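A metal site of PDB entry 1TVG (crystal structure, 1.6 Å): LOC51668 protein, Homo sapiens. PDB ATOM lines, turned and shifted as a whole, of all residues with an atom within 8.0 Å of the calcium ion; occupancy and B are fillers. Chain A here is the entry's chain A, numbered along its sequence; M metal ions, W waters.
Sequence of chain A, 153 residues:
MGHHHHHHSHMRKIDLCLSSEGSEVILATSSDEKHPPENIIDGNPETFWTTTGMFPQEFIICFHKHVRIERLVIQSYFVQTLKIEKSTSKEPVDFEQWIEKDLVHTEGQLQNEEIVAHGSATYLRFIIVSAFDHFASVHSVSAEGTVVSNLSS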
ATOM      1  N   PRO A  36      18.181   0.633 -19.606  1.00  0.00           N
ATOM      2  CA  PRO A  36      18.102   1.939 -18.935  1.00  0.00           C
ATOM      3  C   PRO A  36      17.494   1.917 -17.536  1.00  0.00           C
ATOM      4  O   PRO A  36      16.733   1.013 -17.194  1.00  0.00           O
ATOM      5  CB  PRO A  36      17.280   2.778 -19.907  1.00  0.00           C
ATOM      6  CG  PRO A  36      16.382   1.776 -20.528  1.00  0.00           C
ATOM      7  CD  PRO A  36      17.309   0.607 -20.785  1.00  0.00           C
ATOM      8  N   PRO A  37      17.835   2.922 -16.700  1.00  0.00           N
ATOM      9  CA  PRO A  37      17.333   3.046 -15.332  1.00  0.00           C
ATOM     10  C   PRO A  37      15.813   3.038 -15.256  1.00  0.00           C
ATOM     11  O   PRO A  37      15.232   2.489 -14.320  1.00  0.00           O
ATOM     12  CB  PRO A  37      17.932   4.371 -14.870  1.00  0.00           C
ATOM     13  CG  PRO A  37      19.227   4.411 -15.587  1.00  0.00           C
ATOM     14  CD  PRO A  37      18.861   3.948 -16.980  1.00  0.00           C
ATOM     15  N   GLU A  38      15.166   3.670 -16.229  1.00  0.00           N
ATOM     16  CA  GLU A  38      13.709   3.753 -16.243  1.00  0.00           C
ATOM     17  C   GLU A  38      13.055   2.373 -16.165  1.00  0.00           C
ATOM     18  O   GLU A  38      11.894   2.254 -15.775  1.00  0.00           O
ATOM     19  CB  GLU A  38      13.244   4.498 -17.501  1.00  0.00           C
ATOM     20  CG  GLU A  38      13.529   3.751 -18.795  1.00  0.00           C
ATOM     21  CD  GLU A  38      13.184   4.566 -20.031  1.00  0.00           C
ATOM     22  OE1 GLU A  38      12.048   5.096 -20.101  1.00  0.00           O
ATOM     23  OE2 GLU A  38      14.036   4.657 -20.938  1.00  0.00           O
ATOM     24  N   ASN A  39      13.804   1.334 -16.538  1.00  0.00           N
ATOM     25  CA  ASN A  39      13.305  -0.039 -16.523  1.00  0.00           C
ATOM     26  C   ASN A  39      13.003  -0.540 -15.115  1.00  0.00           C
ATOM     27  O   ASN A  39      12.316  -1.530 -14.942  1.00  0.00           O
ATOM     28  CB  ASN A  39      14.328  -0.995 -17.171  1.00  0.00           C
ATOM     29  CG  ASN A  39      14.268  -0.990 -18.683  1.00  0.00           C
ATOM     30  OD1 ASN A  39      15.054  -1.669 -19.349  1.00  0.00           O
ATOM     31  ND2 ASN A  39      13.326  -0.243 -19.243  1.00  0.00           N
ATOM     32  N   ILE A  40      13.513   0.135 -14.098  1.00  0.00           N
ATOM     33  CA  ILE A  40      13.273  -0.270 -12.723  1.00  0.00           C
ATOM     34  C   ILE A  40      11.845   0.058 -12.249  1.00  0.00           C
ATOM     35  O   ILE A  40      11.316  -0.613 -11.359  1.00  0.00           O
ATOM     36  CB  ILE A  40      14.299   0.413 -11.780  1.00  0.00           C
ATOM     37  CG1 ILE A  40      15.701  -0.086 -12.114  1.00  0.00           C
ATOM     38  CG2 ILE A  40      13.966   0.152 -10.304  1.00  0.00           C
ATOM     39  CD1 ILE A  40      16.809   0.801 -11.574  1.00  0.00           C
ATOM     40  N   ILE A  41      11.226   1.066 -12.850  1.00  0.00           N
ATOM     41  CA  ILE A  41       9.893   1.481 -12.435  1.00  0.00           C
ATOM     42  C   ILE A  41       8.804   1.537 -13.518  1.00  0.00           C
ATOM     43  O   ILE A  41       7.902   2.358 -13.439  1.00  0.00           O
ATOM     44  CB  ILE A  41       9.960   2.850 -11.716  1.00  0.00           C
ATOM     45  CG1 ILE A  41      10.506   3.934 -12.652  1.00  0.00           C
ATOM     46  CG2 ILE A  41      10.878   2.739 -10.505  1.00  0.00           C
ATOM     47  CD1 ILE A  41      10.556   5.326 -12.009  1.00  0.00           C
ATOM     48  N   ASP A  42       8.876   0.649 -14.511  1.00  0.00           N
ATOM     49  CA  ASP A  42       7.875   0.657 -15.572  1.00  0.00           C
ATOM     50  C   ASP A  42       6.780  -0.392 -15.441  1.00  0.00           C
ATOM     51  O   ASP A  42       5.953  -0.548 -16.344  1.00  0.00           O
ATOM     52  CB  ASP A  42       8.552   0.536 -16.941  1.00  0.00           C
ATOM     53  CG  ASP A  42       9.344  -0.746 -17.099  1.00  0.00           C
ATOM     54  OD1 ASP A  42       9.396  -1.545 -16.132  1.00  0.00           O
ATOM     55  OD2 ASP A  42       9.914  -0.970 -18.186  1.00  0.00           O
ATOM     56  N   GLY A  43       6.757  -1.105 -14.318  1.00  0.00           N
ATOM     57  CA  GLY A  43       5.740  -2.103 -14.081  1.00  0.00           C
ATOM     58  C   GLY A  43       5.806  -3.323 -14.984  1.00  0.00           C
ATOM     59  O   GLY A  43       4.803  -4.015 -15.167  1.00  0.00           O
ATOM     60  N   ASN A  44       6.978  -3.590 -15.545  1.00  0.00           N
ATOM     61  CA  ASN A  44       7.158  -4.743 -16.432  1.00  0.00           C
ATOM     62  C   ASN A  44       8.234  -5.644 -15.837  1.00  0.00           C
ATOM     63  O   ASN A  44       9.405  -5.276 -15.800  1.00  0.00           O
ATOM     64  CB  ASN A  44       7.598  -4.260 -17.823  1.00  0.00           C
ATOM     65  CG  ASN A  44       7.720  -5.393 -18.823  1.00  0.00           C
ATOM     66  OD1 ASN A  44       8.174  -6.490 -18.481  1.00  0.00           O
ATOM     67  ND2 ASN A  44       7.346  -5.138 -20.072  1.00  0.00           N
ATOM     68  N   PRO A  45       7.870  -6.849 -15.385  1.00  0.00           N
ATOM     69  CA  PRO A  45       8.864  -7.752 -14.801  1.00  0.00           C
ATOM     70  C   PRO A  45      10.013  -8.186 -15.706  1.00  0.00           C
ATOM     71  O   PRO A  45      11.066  -8.556 -15.213  1.00  0.00           O
ATOM     72  CB  PRO A  45       8.022  -8.926 -14.321  1.00  0.00           C
ATOM     73  CG  PRO A  45       6.919  -8.951 -15.291  1.00  0.00           C
ATOM     74  CD  PRO A  45       6.551  -7.494 -15.447  1.00  0.00           C
ATOM     75  N   GLU A  46       9.846  -8.141 -17.031  1.00  0.00           N
ATOM     76  CA  GLU A  46      10.971  -8.581 -17.848  1.00  0.00           C
ATOM     77  C   GLU A  46      11.993  -7.525 -18.283  1.00  0.00           C
ATOM     78  O   GLU A  46      13.099  -7.869 -18.681  1.00  0.00           O
ATOM     79  CB  GLU A  46      10.511  -9.425 -19.048  1.00  0.00           C
ATOM     80  CG  GLU A  46       9.519  -8.858 -20.029  1.00  0.00           C
ATOM     81  CD  GLU A  46       9.311  -9.821 -21.209  1.00  0.00           C
ATOM     82  OE1 GLU A  46       9.342 -11.046 -20.973  1.00  0.00           O
ATOM     83  OE2 GLU A  46       9.132  -9.366 -22.348  1.00  0.00           O
ATOM     84  N   THR A  47      11.656  -6.237 -18.171  1.00  0.00           N
ATOM     85  CA  THR A  47      12.635  -5.205 -18.502  1.00  0.00           C
ATOM     86  C   THR A  47      13.435  -4.909 -17.248  1.00  0.00           C
ATOM     87  O   THR A  47      12.901  -4.933 -16.138  1.00  0.00           O
ATOM     88  CB  THR A  47      11.972  -3.887 -18.959  1.00  0.00           C
ATOM     89  OG1 THR A  47      11.162  -3.361 -17.902  1.00  0.00           O
ATOM     90  CG2 THR A  47      11.090  -4.125 -20.171  1.00  0.00           C
ATOM     91  N   PHE A  48      14.722  -4.626 -17.407  1.00  0.00           N
ATOM     92  CA  PHE A  48      15.554  -4.357 -16.245  1.00  0.00           C
ATOM     93  C   PHE A  48      16.725  -3.423 -16.511  1.00  0.00           C
ATOM     94  O   PHE A  48      17.099  -3.160 -17.657  1.00  0.00           O
ATOM     95  CB  PHE A  48      16.113  -5.660 -15.680  1.00  0.00           C
ATOM     96  CG  PHE A  48      16.909  -6.468 -16.673  1.00  0.00           C
ATOM     97  CD1 PHE A  48      16.272  -7.318 -17.572  1.00  0.00           C
ATOM     98  CD2 PHE A  48      18.307  -6.398 -16.703  1.00  0.00           C
ATOM     99  CE1 PHE A  48      17.004  -8.086 -18.484  1.00  0.00           C
ATOM    100  CE2 PHE A  48      19.046  -7.161 -17.608  1.00  0.00           C
ATOM    101  CZ  PHE A  48      18.398  -8.009 -18.499  1.00  0.00           C
ATOM    102  N   TRP A  49      17.270  -2.912 -15.417  1.00  0.00           N
ATOM    103  CA  TRP A  49      18.454  -2.052 -15.445  1.00  0.00           C
ATOM    104  C   TRP A  49      19.560  -3.009 -15.027  1.00  0.00           C
ATOM    105  O   TRP A  49      19.360  -3.849 -14.143  1.00  0.00           O
ATOM    106  CB  TRP A  49      18.325  -0.929 -14.416  1.00  0.00           C
ATOM    107  CG  TRP A  49      19.610  -0.173 -14.132  1.00  0.00           C
ATOM    108  CD1 TRP A  49      20.180   0.792 -14.918  1.00  0.00           C
ATOM    109  CD2 TRP A  49      20.442  -0.310 -12.975  1.00  0.00           C
ATOM    110  NE1 TRP A  49      21.320   1.277 -14.310  1.00  0.00           N
ATOM    111  CE2 TRP A  49      21.511   0.615 -13.121  1.00  0.00           C
ATOM    112  CE3 TRP A  49      20.400  -1.107 -11.824  1.00  0.00           C
ATOM    113  CZ2 TRP A  49      22.515   0.767 -12.155  1.00  0.00           C
ATOM    114  CZ3 TRP A  49      21.404  -0.967 -10.866  1.00  0.00           C
ATOM    115  CH2 TRP A  49      22.441  -0.040 -11.044  1.00  0.00           C
ATOM    116  N   GLN A  75      12.536  -6.876  -7.233  1.00  0.00           N
ATOM    117  CA  GLN A  75      12.692  -8.006  -8.145  1.00  0.00           C
ATOM    118  C   GLN A  75      14.041  -7.771  -8.813  1.00  0.00           C
ATOM    119  O   GLN A  75      14.233  -6.748  -9.455  1.00  0.00           O
ATOM    120  CB  GLN A  75      11.593  -7.990  -9.192  1.00  0.00           C
ATOM    121  CG  GLN A  75      11.385  -9.310  -9.884  1.00  0.00           C
ATOM    122  CD  GLN A  75      10.240  -9.264 -10.861  1.00  0.00           C
ATOM    123  OE1 GLN A  75      10.381  -8.767 -11.984  1.00  0.00           O
ATOM    124  NE2 GLN A  75       9.080  -9.765 -10.447  1.00  0.00           N
ATOM    125  N   VAL A 138      18.325  -5.171 -11.794  1.00  0.00           N
ATOM    126  CA  VAL A 138      17.149  -4.831 -11.031  1.00  0.00           C
ATOM    127  C   VAL A 138      15.983  -4.737 -12.003  1.00  0.00           C
ATOM    128  O   VAL A 138      15.944  -3.876 -12.870  1.00  0.00           O
ATOM    129  CB  VAL A 138      17.303  -3.484 -10.289  1.00  0.00           C
ATOM    130  CG1 VAL A 138      15.965  -3.091  -9.652  1.00  0.00           C
ATOM    131  CG2 VAL A 138      18.368  -3.611  -9.212  1.00  0.00           C
ATOM    132  N   HIS A 139      15.043  -5.661 -11.845  1.00  0.00           N
ATOM    133  CA  HIS A 139      13.869  -5.720 -12.707  1.00  0.00           C
ATOM    134  C   HIS A 139      12.764  -4.766 -12.255  1.00  0.00           C
ATOM    135  O   HIS A 139      12.108  -4.138 -13.077  1.00  0.00           O
ATOM    136  CB  HIS A 139      13.324  -7.153 -12.731  1.00  0.00           C
ATOM    137  CG  HIS A 139      14.129  -8.076 -13.592  1.00  0.00           C
ATOM    138  ND1 HIS A 139      15.471  -8.308 -13.396  1.00  0.00           N
ATOM    139  CD2 HIS A 139      13.774  -8.810 -14.675  1.00  0.00           C
ATOM    140  CE1 HIS A 139      15.916  -9.143 -14.322  1.00  0.00           C
ATOM    141  NE2 HIS A 139      14.907  -9.454 -15.114  1.00  0.00           N
ATOM    142  N   SER A 140      12.564  -4.657 -10.956  1.00  0.00           N
ATOM    143  CA  SER A 140      11.531  -3.782 -10.444  1.00  0.00           C
ATOM    144  C   SER A 140      11.745  -3.440  -8.992  1.00  0.00           C
ATOM    145  O   SER A 140      12.314  -4.225  -8.227  1.00  0.00           O
ATOM    146  CB  SER A 140      10.167  -4.440 -10.594  1.00  0.00           C
ATOM    147  OG  SER A 140       9.127  -3.611 -10.075  1.00  0.00           O
ATOM    148  N   VAL A 141      11.298  -2.241  -8.618  1.00  0.00           N
ATOM    149  CA  VAL A 141      11.353  -1.786  -7.241  1.00  0.00           C
ATOM    150  C   VAL A 141       9.985  -1.177  -7.015  1.00  0.00           C
ATOM    151  O   VAL A 141       9.551  -0.284  -7.751  1.00  0.00           O
ATOM    152  CB  VAL A 141      12.443  -0.728  -7.001  1.00  0.00           C
ATOM    153  CG1 VAL A 141      12.220  -0.069  -5.645  1.00  0.00           C
ATOM    154  CG2 VAL A 141      13.808  -1.408  -7.021  1.00  0.00           C
HETATM  155 CA    CA M   1      10.976  -3.466 -15.263  1.00  0.00          CA
HETATM  156  O   HOH W   1       9.168  -3.166 -13.391  1.00  0.00           O
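The backbone NH of Glu 46 sits at hydrogen-bond distance from the side-chain amide oxygen of Asn 44 (2.8 Å).
The side-chain amide oxygen of Asn 39 sits close to the backbone carbonyl oxygen of Phe 48.
N of His 139 is in hydrogen-bond range of O of Gln 75 (2.7 Å).
Five residues have an atom within 4 Å of the calcium ion: Asn 39, Asp 42, Asn 44, Thr 47 and His 139.
The nearest printed residue that does not touch the calcium ion is Phe 48 (4.5 Å).
The calcium ion is bound by the backbone carbonyl oxygen (O) of Asn 39 (2.4 Å), the backbone carbonyl oxygen (O) of Asn 44 (2.5 Å), the backbone carbonyl oxygen (O) of His 139 (2.6 Å), the backbone carbonyl oxygen (O) of Thr 47 (2.6 Å), water W1 (2.6 Å), the side-chain carboxylate (OD1) of Asp 42 (2.6 Å) and the side-chain hydroxyl (OG1) of Thr 47 (2.6 Å).
The calcium ion has seven donor atoms within binding distance.
Water W1 lies within hydrogen-bond range of N of Asn 44 (3.1 Å), N of Gly 43 (3.3 Å) and OG of Ser 140 (3.3 Å).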
